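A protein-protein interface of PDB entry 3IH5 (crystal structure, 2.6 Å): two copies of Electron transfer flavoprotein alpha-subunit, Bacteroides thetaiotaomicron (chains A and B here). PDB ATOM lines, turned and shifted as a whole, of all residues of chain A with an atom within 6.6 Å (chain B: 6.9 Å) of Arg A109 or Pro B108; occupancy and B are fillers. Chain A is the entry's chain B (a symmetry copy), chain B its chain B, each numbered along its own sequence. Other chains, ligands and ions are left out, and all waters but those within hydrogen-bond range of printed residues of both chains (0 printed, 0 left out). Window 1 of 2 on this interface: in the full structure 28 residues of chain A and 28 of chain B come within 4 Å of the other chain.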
ATOM      1  N   TYR A  74      23.021  14.208   4.868  1.00  0.00           N
ATOM      2  CA  TYR A  74      23.097  12.808   5.206  1.00  0.00           C
ATOM      3  C   TYR A  74      22.015  11.991   4.494  1.00  0.00           C
ATOM      4  O   TYR A  74      20.850  12.382   4.462  1.00  0.00           O
ATOM      5  CB  TYR A  74      22.950  12.660   6.722  1.00  0.00           C
ATOM      6  CG  TYR A  74      22.846  11.228   7.184  1.00  0.00           C
ATOM      7  CD1 TYR A  74      21.615  10.609   7.311  1.00  0.00           C
ATOM      8  CD2 TYR A  74      23.980  10.494   7.474  1.00  0.00           C
ATOM      9  CE1 TYR A  74      21.513   9.292   7.716  1.00  0.00           C
ATOM     10  CE2 TYR A  74      23.894   9.182   7.884  1.00  0.00           C
ATOM     11  CZ  TYR A  74      22.658   8.582   8.002  1.00  0.00           C
ATOM     12  OH  TYR A  74      22.569   7.274   8.413  1.00  0.00           O
ATOM     13  N   SER A  76      21.200   7.519   4.214  1.00  0.00           N
ATOM     14  CA  SER A  76      21.626   6.363   4.996  1.00  0.00           C
ATOM     15  C   SER A  76      22.626   5.472   4.282  1.00  0.00           C
ATOM     16  O   SER A  76      23.589   5.007   4.881  1.00  0.00           O
ATOM     17  CB  SER A  76      20.421   5.544   5.466  1.00  0.00           C
ATOM     18  OG  SER A  76      19.444   6.384   6.057  1.00  0.00           O
ATOM     19  N   LEU A  77      22.406   5.241   2.999  1.00  0.00           N
ATOM     20  CA  LEU A  77      23.184   4.248   2.277  1.00  0.00           C
ATOM     21  C   LEU A  77      24.659   4.645   2.105  1.00  0.00           C
ATOM     22  O   LEU A  77      25.547   3.839   2.392  1.00  0.00           O
ATOM     23  CB  LEU A  77      22.524   3.951   0.934  1.00  0.00           C
ATOM     24  CG  LEU A  77      22.537   2.486   0.514  1.00  0.00           C
ATOM     25  CD1 LEU A  77      23.830   2.153  -0.207  1.00  0.00           C
ATOM     26  CD2 LEU A  77      22.319   1.585   1.726  1.00  0.00           C
ATOM     27  N   THR A  80      26.438   4.778   5.529  1.00  0.00           N
ATOM     28  CA  THR A  80      26.493   3.418   6.054  1.00  0.00           C
ATOM     29  C   THR A  80      27.593   2.604   5.384  1.00  0.00           C
ATOM     30  O   THR A  80      28.397   1.964   6.063  1.00  0.00           O
ATOM     31  CB  THR A  80      25.154   2.682   5.882  1.00  0.00           C
ATOM     32  OG1 THR A  80      24.150   3.334   6.662  1.00  0.00           O
ATOM     33  CG2 THR A  80      25.277   1.245   6.343  1.00  0.00           C
ATOM     34  N   VAL A  84      30.912   0.939   7.046  1.00  0.00           N
ATOM     35  CA  VAL A  84      31.013  -0.519   6.970  1.00  0.00           C
ATOM     36  C   VAL A  84      32.291  -0.941   6.259  1.00  0.00           C
ATOM     37  O   VAL A  84      32.980  -1.864   6.690  1.00  0.00           O
ATOM     38  CB  VAL A  84      29.792  -1.173   6.271  1.00  0.00           C
ATOM     39  CG1 VAL A  84      30.060  -2.649   6.024  1.00  0.00           C
ATOM     40  CG2 VAL A  84      28.529  -1.005   7.110  1.00  0.00           C
ATOM     41  N   ARG A 104      20.675   7.636  15.365  1.00  0.00           N
ATOM     42  CA  ARG A 104      19.582   6.698  15.506  1.00  0.00           C
ATOM     43  C   ARG A 104      19.298   5.970  14.202  1.00  0.00           C
ATOM     44  O   ARG A 104      18.668   4.911  14.207  1.00  0.00           O
ATOM     45  CB  ARG A 104      18.337   7.392  16.052  1.00  0.00           C
ATOM     46  CG  ARG A 104      18.168   7.206  17.545  1.00  0.00           C
ATOM     47  CD  ARG A 104      17.062   8.060  18.123  1.00  0.00           C
ATOM     48  NE  ARG A 104      17.614   9.210  18.832  1.00  0.00           N
ATOM     49  CZ  ARG A 104      17.498  10.466  18.417  1.00  0.00           C
ATOM     50  NH1 ARG A 104      16.835  10.739  17.303  1.00  0.00           N
ATOM     51  NH2 ARG A 104      18.032  11.447  19.121  1.00  0.00           N
ATOM     52  N   ASP A 105      19.779   6.518  13.091  1.00  0.00           N
ATOM     53  CA  ASP A 105      19.679   5.814  11.813  1.00  0.00           C
ATOM     54  C   ASP A 105      20.944   5.033  11.474  1.00  0.00           C
ATOM     55  O   ASP A 105      20.892   3.839  11.190  1.00  0.00           O
ATOM     56  CB  ASP A 105      19.382   6.783  10.672  1.00  0.00           C
ATOM     57  CG  ASP A 105      19.171   6.065   9.344  1.00  0.00           C
ATOM     58  OD1 ASP A 105      18.096   5.449   9.152  1.00  0.00           O
ATOM     59  OD2 ASP A 105      20.084   6.114   8.496  1.00  0.00           O
ATOM     60  N   LEU A 106      22.080   5.720  11.501  1.00  0.00           N
ATOM     61  CA  LEU A 106      23.341   5.147  11.056  1.00  0.00           C
ATOM     62  C   LEU A 106      23.798   3.977  11.931  1.00  0.00           C
ATOM     63  O   LEU A 106      24.300   2.968  11.423  1.00  0.00           O
ATOM     64  CB  LEU A 106      24.418   6.240  11.002  1.00  0.00           C
ATOM     65  CG  LEU A 106      25.779   5.837  10.433  1.00  0.00           C
ATOM     66  CD1 LEU A 106      25.663   5.541   8.951  1.00  0.00           C
ATOM     67  CD2 LEU A 106      26.819   6.922  10.681  1.00  0.00           C
ATOM     68  N   GLY A 107      23.623   4.113  13.244  1.00  0.00           N
ATOM     69  CA  GLY A 107      24.079   3.106  14.187  1.00  0.00           C
ATOM     70  C   GLY A 107      23.600   1.705  13.854  1.00  0.00           C
ATOM     71  O   GLY A 107      24.419   0.818  13.580  1.00  0.00           O
ATOM     72  N   PRO A 108      22.268   1.496  13.883  1.00  0.00           N
ATOM     73  CA  PRO A 108      21.627   0.210  13.583  1.00  0.00           C
ATOM     74  C   PRO A 108      22.047  -0.391  12.248  1.00  0.00           C
ATOM     75  O   PRO A 108      22.283  -1.602  12.172  1.00  0.00           O
ATOM     76  CB  PRO A 108      20.136   0.559  13.570  1.00  0.00           C
ATOM     77  CG  PRO A 108      20.026   1.676  14.565  1.00  0.00           C
ATOM     78  CD  PRO A 108      21.292   2.491  14.369  1.00  0.00           C
ATOM     79  N   ARG A 109      22.132   0.423  11.202  1.00  0.00           N
ATOM     80  CA  ARG A 109      22.554  -0.118   9.917  1.00  0.00           C
ATOM     81  C   ARG A 109      23.992  -0.618   9.968  1.00  0.00           C
ATOM     82  O   ARG A 109      24.253  -1.780   9.641  1.00  0.00           O
ATOM     83  CB  ARG A 109      22.378   0.898   8.798  1.00  0.00           C
ATOM     84  CG  ARG A 109      20.972   1.410   8.644  1.00  0.00           C
ATOM     85  CD  ARG A 109      20.993   2.656   7.814  1.00  0.00           C
ATOM     86  NE  ARG A 109      19.683   3.279   7.677  1.00  0.00           N
ATOM     87  CZ  ARG A 109      18.759   2.873   6.813  1.00  0.00           C
ATOM     88  NH1 ARG A 109      17.594   3.509   6.736  1.00  0.00           N
ATOM     89  NH2 ARG A 109      19.002   1.829   6.034  1.00  0.00           N
ATOM     90  N   VAL A 110      24.921   0.237  10.401  1.00  0.00           N
ATOM     91  CA  VAL A 110      26.334  -0.163  10.454  1.00  0.00           C
ATOM     92  C   VAL A 110      26.570  -1.390  11.353  1.00  0.00           C
ATOM     93  O   VAL A 110      27.262  -2.334  10.957  1.00  0.00           O
ATOM     94  CB  VAL A 110      27.276   1.007  10.838  1.00  0.00           C
ATOM     95  CG1 VAL A 110      28.681   0.499  11.010  1.00  0.00           C
ATOM     96  CG2 VAL A 110      27.243   2.082   9.762  1.00  0.00           C
ATOM     97  N   SER A 111      25.975  -1.401  12.543  1.00  0.00           N
ATOM     98  CA  SER A 111      26.115  -2.554  13.424  1.00  0.00           C
ATOM     99  C   SER A 111      25.550  -3.850  12.822  1.00  0.00           C
ATOM    100  O   SER A 111      26.165  -4.912  12.946  1.00  0.00           O
ATOM    101  CB  SER A 111      25.486  -2.272  14.782  1.00  0.00           C
ATOM    102  OG  SER A 111      24.186  -1.747  14.623  1.00  0.00           O
ATOM    103  N   SER A 112      24.389  -3.761  12.172  1.00  0.00           N
ATOM    104  CA  SER A 112      23.775  -4.927  11.520  1.00  0.00           C
ATOM    105  C   SER A 112      24.670  -5.463  10.412  1.00  0.00           C
ATOM    106  O   SER A 112      24.804  -6.676  10.248  1.00  0.00           O
ATOM    107  CB  SER A 112      22.401  -4.577  10.935  1.00  0.00           C
ATOM    108  OG  SER A 112      21.403  -4.505  11.939  1.00  0.00           O
ATOM    109  N   ALA A 113      25.283  -4.552   9.658  1.00  0.00           N
ATOM    110  CA  ALA A 113      26.116  -4.922   8.517  1.00  0.00           C
ATOM    111  C   ALA A 113      27.432  -5.537   8.959  1.00  0.00           C
ATOM    112  O   ALA A 113      28.016  -6.336   8.229  1.00  0.00           O
ATOM    113  CB  ALA A 113      26.378  -3.717   7.633  1.00  0.00           C
ATOM    114  N   LEU A 114      27.903  -5.153  10.145  1.00  0.00           N
ATOM    115  CA  LEU A 114      29.153  -5.685  10.677  1.00  0.00           C
ATOM    116  C   LEU A 114      28.869  -6.798  11.675  1.00  0.00           C
ATOM    117  O   LEU A 114      29.783  -7.329  12.318  1.00  0.00           O
ATOM    118  CB  LEU A 114      29.990  -4.576  11.323  1.00  0.00           C
ATOM    119  CG  LEU A 114      30.378  -3.435  10.380  1.00  0.00           C
ATOM    120  CD1 LEU A 114      30.989  -2.275  11.146  1.00  0.00           C
ATOM    121  CD2 LEU A 114      31.325  -3.925   9.294  1.00  0.00           C
ATOM    122  N   LEU A 118      25.608  -2.823  19.721  1.00  0.00           N
ATOM    123  CA  LEU A 118      25.301  -1.400  19.764  1.00  0.00           C
ATOM    124  C   LEU A 118      24.466  -1.095  21.000  1.00  0.00           C
ATOM    125  O   LEU A 118      23.345  -1.588  21.130  1.00  0.00           O
ATOM    126  CB  LEU A 118      24.508  -0.990  18.526  1.00  0.00           C
ATOM    127  CG  LEU A 118      24.191   0.504  18.482  1.00  0.00           C
ATOM    128  CD1 LEU A 118      25.402   1.244  17.973  1.00  0.00           C
ATOM    129  CD2 LEU A 118      23.014   0.781  17.586  1.00  0.00           C
ATOM    130  N   MET B  97       7.784  -7.383   2.468  1.00  0.00           N
ATOM    131  CA  MET B  97       7.403  -7.665   3.845  1.00  0.00           C
ATOM    132  C   MET B  97       6.411  -6.641   4.375  1.00  0.00           C
ATOM    133  O   MET B  97       6.264  -5.547   3.822  1.00  0.00           O
ATOM    134  CB  MET B  97       8.628  -7.764   4.770  1.00  0.00           C
ATOM    135  CG  MET B  97       9.463  -6.495   4.892  1.00  0.00           C
ATOM    136  SD  MET B  97      11.195  -6.827   5.764  1.00  0.00           S
ATOM    137  CE  MET B  97      10.644  -6.720   7.605  1.00  0.00           C
ATOM    138  N   ILE B 102       8.019  -4.944  13.125  1.00  0.00           N
ATOM    139  CA  ILE B 102       9.137  -5.775  12.713  1.00  0.00           C
ATOM    140  C   ILE B 102       9.649  -5.361  11.336  1.00  0.00           C
ATOM    141  O   ILE B 102      10.853  -5.304  11.096  1.00  0.00           O
ATOM    142  CB  ILE B 102       8.739  -7.256  12.711  1.00  0.00           C
ATOM    143  CG1 ILE B 102       8.590  -7.747  14.153  1.00  0.00           C
ATOM    144  CG2 ILE B 102       9.743  -8.089  11.920  1.00  0.00           C
ATOM    145  CD1 ILE B 102       8.228  -9.194  14.273  1.00  0.00           C
ATOM    146  N   GLY B 103       8.733  -5.062  10.433  1.00  0.00           N
ATOM    147  CA  GLY B 103       9.128  -4.586   9.125  1.00  0.00           C
ATOM    148  C   GLY B 103       9.924  -3.297   9.183  1.00  0.00           C
ATOM    149  O   GLY B 103      10.926  -3.125   8.477  1.00  0.00           O
ATOM    150  N   ARG B 104       9.460  -2.380  10.025  1.00  0.00           N
ATOM    151  CA  ARG B 104      10.104  -1.093  10.171  1.00  0.00           C
ATOM    152  C   ARG B 104      11.496  -1.228  10.767  1.00  0.00           C
ATOM    153  O   ARG B 104      12.316  -0.317  10.641  1.00  0.00           O
ATOM    154  CB  ARG B 104       9.231  -0.135  10.977  1.00  0.00           C
ATOM    155  CG  ARG B 104       8.430   0.807  10.103  1.00  0.00           C
ATOM    156  CD  ARG B 104       7.411   1.609  10.881  1.00  0.00           C
ATOM    157  NE  ARG B 104       6.068   1.075  10.677  1.00  0.00           N
ATOM    158  CZ  ARG B 104       5.360   0.462  11.618  1.00  0.00           C
ATOM    159  NH1 ARG B 104       5.860   0.316  12.837  1.00  0.00           N
ATOM    160  NH2 ARG B 104       4.152   0.006  11.344  1.00  0.00           N
ATOM    161  N   ASP B 105      11.772  -2.366  11.396  1.00  0.00           N
ATOM    162  CA  ASP B 105      13.127  -2.640  11.872  1.00  0.00           C
ATOM    163  C   ASP B 105      13.937  -3.477  10.887  1.00  0.00           C
ATOM    164  O   ASP B 105      15.041  -3.103  10.500  1.00  0.00           O
ATOM    165  CB  ASP B 105      13.103  -3.359  13.219  1.00  0.00           C
ATOM    166  CG  ASP B 105      14.501  -3.567  13.789  1.00  0.00           C
ATOM    167  OD1 ASP B 105      15.107  -2.585  14.280  1.00  0.00           O
ATOM    168  OD2 ASP B 105      14.993  -4.711  13.740  1.00  0.00           O
ATOM    169  N   LEU B 106      13.379  -4.615  10.491  1.00  0.00           N
ATOM    170  CA  LEU B 106      14.095  -5.582   9.674  1.00  0.00           C
ATOM    171  C   LEU B 106      14.442  -5.039   8.286  1.00  0.00           C
ATOM    172  O   LEU B 106      15.541  -5.278   7.772  1.00  0.00           O
ATOM    173  CB  LEU B 106      13.276  -6.876   9.563  1.00  0.00           C
ATOM    174  CG  LEU B 106      13.938  -8.050   8.841  1.00  0.00           C
ATOM    175  CD1 LEU B 106      15.107  -8.575   9.651  1.00  0.00           C
ATOM    176  CD2 LEU B 106      12.934  -9.164   8.570  1.00  0.00           C
ATOM    177  N   GLY B 107      13.507  -4.310   7.681  1.00  0.00           N
ATOM    178  CA  GLY B 107      13.686  -3.798   6.333  1.00  0.00           C
ATOM    179  C   GLY B 107      14.984  -3.035   6.143  1.00  0.00           C
ATOM    180  O   GLY B 107      15.838  -3.452   5.350  1.00  0.00           O
ATOM    181  N   PRO B 108      15.137  -1.907   6.867  1.00  0.00           N
ATOM    182  CA  PRO B 108      16.327  -1.049   6.817  1.00  0.00           C
ATOM    183  C   PRO B 108      17.634  -1.795   7.049  1.00  0.00           C
ATOM    184  O   PRO B 108      18.617  -1.534   6.347  1.00  0.00           O
ATOM    185  CB  PRO B 108      16.077  -0.041   7.942  1.00  0.00           C
ATOM    186  CG  PRO B 108      14.582   0.093   7.970  1.00  0.00           C
ATOM    187  CD  PRO B 108      14.067  -1.307   7.687  1.00  0.00           C
ATOM    188  N   ARG B 109      17.666  -2.700   8.020  1.00  0.00           N
ATOM    189  CA  ARG B 109      18.896  -3.446   8.252  1.00  0.00           C
ATOM    190  C   ARG B 109      19.240  -4.335   7.063  1.00  0.00           C
ATOM    191  O   ARG B 109      20.344  -4.237   6.518  1.00  0.00           O
ATOM    192  CB  ARG B 109      18.821  -4.266   9.531  1.00  0.00           C
ATOM    193  CG  ARG B 109      18.532  -3.457  10.766  1.00  0.00           C
ATOM    194  CD  ARG B 109      18.093  -4.378  11.862  1.00  0.00           C
ATOM    195  NE  ARG B 109      17.708  -3.680  13.082  1.00  0.00           N
ATOM    196  CZ  ARG B 109      18.577  -3.230  13.981  1.00  0.00           C
ATOM    197  NH1 ARG B 109      18.142  -2.619  15.079  1.00  0.00           N
ATOM    198  NH2 ARG B 109      19.876  -3.388  13.776  1.00  0.00           N
ATOM    199  N   VAL B 110      18.298  -5.180   6.639  1.00  0.00           N
ATOM    200  CA  VAL B 110      18.562  -6.088   5.515  1.00  0.00           C
ATOM    201  C   VAL B 110      18.941  -5.339   4.223  1.00  0.00           C
ATOM    202  O   VAL B 110      19.917  -5.696   3.555  1.00  0.00           O
ATOM    203  CB  VAL B 110      17.407  -7.092   5.267  1.00  0.00           C
ATOM    204  CG1 VAL B 110      17.681  -7.892   4.023  1.00  0.00           C
ATOM    205  CG2 VAL B 110      17.257  -8.024   6.458  1.00  0.00           C
ATOM    206  N   SER B 111      18.199  -4.287   3.885  1.00  0.00           N
ATOM    207  CA  SER B 111      18.533  -3.503   2.703  1.00  0.00           C
ATOM    208  C   SER B 111      19.921  -2.848   2.779  1.00  0.00           C
ATOM    209  O   SER B 111      20.660  -2.842   1.792  1.00  0.00           O
ATOM    210  CB  SER B 111      17.458  -2.457   2.432  1.00  0.00           C
ATOM    211  OG  SER B 111      17.163  -1.739   3.609  1.00  0.00           O
ATOM    212  N   SER B 112      20.273  -2.307   3.946  1.00  0.00           N
ATOM    213  CA  SER B 112      21.592  -1.691   4.149  1.00  0.00           C
ATOM    214  C   SER B 112      22.703  -2.718   3.976  1.00  0.00           C
ATOM    215  O   SER B 112      23.744  -2.421   3.390  1.00  0.00           O
ATOM    216  CB  SER B 112      21.703  -1.056   5.539  1.00  0.00           C
ATOM    217  OG  SER B 112      21.017   0.184   5.609  1.00  0.00           O
ATOM    218  N   ALA B 113      22.470  -3.926   4.487  1.00  0.00           N
ATOM    219  CA  ALA B 113      23.473  -4.987   4.456  1.00  0.00           C
ATOM    220  C   ALA B 113      23.659  -5.542   3.055  1.00  0.00           C
ATOM    221  O   ALA B 113      24.736  -6.038   2.726  1.00  0.00           O
ATOM    222  CB  ALA B 113      23.099  -6.104   5.411  1.00  0.00           C
ATOM    223  N   LEU B 118      14.755   0.106  -0.859  1.00  0.00           N
ATOM    224  CA  LEU B 118      13.629  -0.200   0.012  1.00  0.00           C
ATOM    225  C   LEU B 118      12.617   0.935  -0.044  1.00  0.00           C
ATOM    226  O   LEU B 118      12.923   2.063   0.345  1.00  0.00           O
ATOM    227  CB  LEU B 118      14.102  -0.361   1.455  1.00  0.00           C
ATOM    228  CG  LEU B 118      12.977  -0.730   2.419  1.00  0.00           C
ATOM    229  CD1 LEU B 118      12.718  -2.212   2.321  1.00  0.00           C
ATOM    230  CD2 LEU B 118      13.339  -0.372   3.836  1.00  0.00           C
ATOM    231  N   MET B 167      13.209  -4.108  -2.794  1.00  0.00           N
ATOM    232  CA  MET B 167      12.471  -4.400  -1.568  1.00  0.00           C
ATOM    233  C   MET B 167      11.383  -3.374  -1.309  1.00  0.00           C
ATOM    234  O   MET B 167      11.540  -2.197  -1.623  1.00  0.00           O
ATOM    235  CB  MET B 167      13.417  -4.475  -0.371  1.00  0.00           C
ATOM    236  CG  MET B 167      14.499  -5.544  -0.488  1.00  0.00           C
ATOM    237  SD  MET B 167      15.571  -5.743   1.139  1.00  0.00           S
ATOM    238  CE  MET B 167      14.138  -5.793   2.459  1.00  0.00           C
ATOM    239  N   THR B 169       7.686  -2.561   1.410  1.00  0.00           N
ATOM    240  CA  THR B 169       6.813  -2.956   2.494  1.00  0.00           C
ATOM    241  C   THR B 169       5.421  -2.427   2.204  1.00  0.00           C
ATOM    242  O   THR B 169       5.255  -1.463   1.460  1.00  0.00           O
ATOM    243  CB  THR B 169       7.308  -2.421   3.855  1.00  0.00           C
ATOM    244  OG1 THR B 169       7.307  -0.987   3.834  1.00  0.00           O
ATOM    245  CG2 THR B 169       8.711  -2.929   4.150  1.00  0.00           C
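Of chain B, only Pro B108 (3.4 Å) and Ser B112 (2.6 Å) come within 4 Å of Arg A109.
Printed residues of chain A within 4 Å of Pro B108: Arg A109.
Printed residues of chain A within 4 Å of Arg B109: Pro A108 and Ser A112.
Of the printed residues of chain B, Pro A108 touches Arg B109 (3.4 Å).
Of the printed residues of chain B, Ser A112 touches Arg B109 (2.6 Å).
Ala A113 touches none of the printed residues of chain B.
Ile B102 touches none of the printed residues of chain A.
The nearest residue of chain B that does not touch Arg A109 is Ser B111 (4.7 Å).
The nearest residue of chain A that does not touch Pro B108 is Asp A105 (6.0 Å).
The nearest printed residue of chain B that does not touch Ser A112 is Ala B113 (5.2 Å).
The backbone carbonyl oxygen (O) of Pro B108 lies within hydrogen-bond range of the guanidinium group (NH2) of Arg A109 (3.4 Å).
O of Pro A108 sits at hydrogen-bond distance from NH2 of Arg B109 (3.4 Å).
OG of Ser A112 sits at hydrogen-bond distance from NH2 of Arg B109, at 2.6 Å.
The side-chain hydroxyl of Ser B112 sits at hydrogen-bond distance from the guanidinium group of Arg A109.
Pro A108 touches Arg B109, and with the chains exchanged Arg A109 touches Pro B108.
Arg A109 touches Ser B112, and with the chains exchanged Ser A112 touches Arg B109.
Of the 4 pairs that touch across the chains among the printed residues, 4 have their exchanged pair printed and touching as well.
The side-chain carboxylate (OD2) of Asp B105 is in salt-bridge range of the guanidinium group (NE) of Arg B109 (3.0 Å).
The side-chain hydroxyl (OG) of Ser B111 is in hydrogen-bond range of the backbone carbonyl oxygen (O) of Pro B108, at 3.1 Å.
The backbone carbonyl oxygen (O) of Pro B108 is in hydrogen-bond range of the side-chain hydroxyl (OG) of Ser B112.
OG of Ser A76 sits at hydrogen-bond distance from NH1 of Arg A109 (3.5 Å).
The side-chain carboxylate (OD2) of Asp A105 lies within salt-bridge range of the guanidinium group (NE) of Arg A109 (3.0 Å).
OG of Ser A111 lies within hydrogen-bond range of O of Pro A108.
Printed residues of chain A that touch a printed residue of chain B: Pro A108, Arg A109 and Ser A112.
Of the 16 printed residues of chain B, 3 touch a printed residue of chain A.
Printed residues of chain B that touch a printed residue of chain A: Pro B108, Arg B109 and Ser B112.
Hydrophobic or aromatic side chains of chain B that line the printed part of chain A: Pro B108.
Among the printed residues, 4 pairs touch across the chains.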
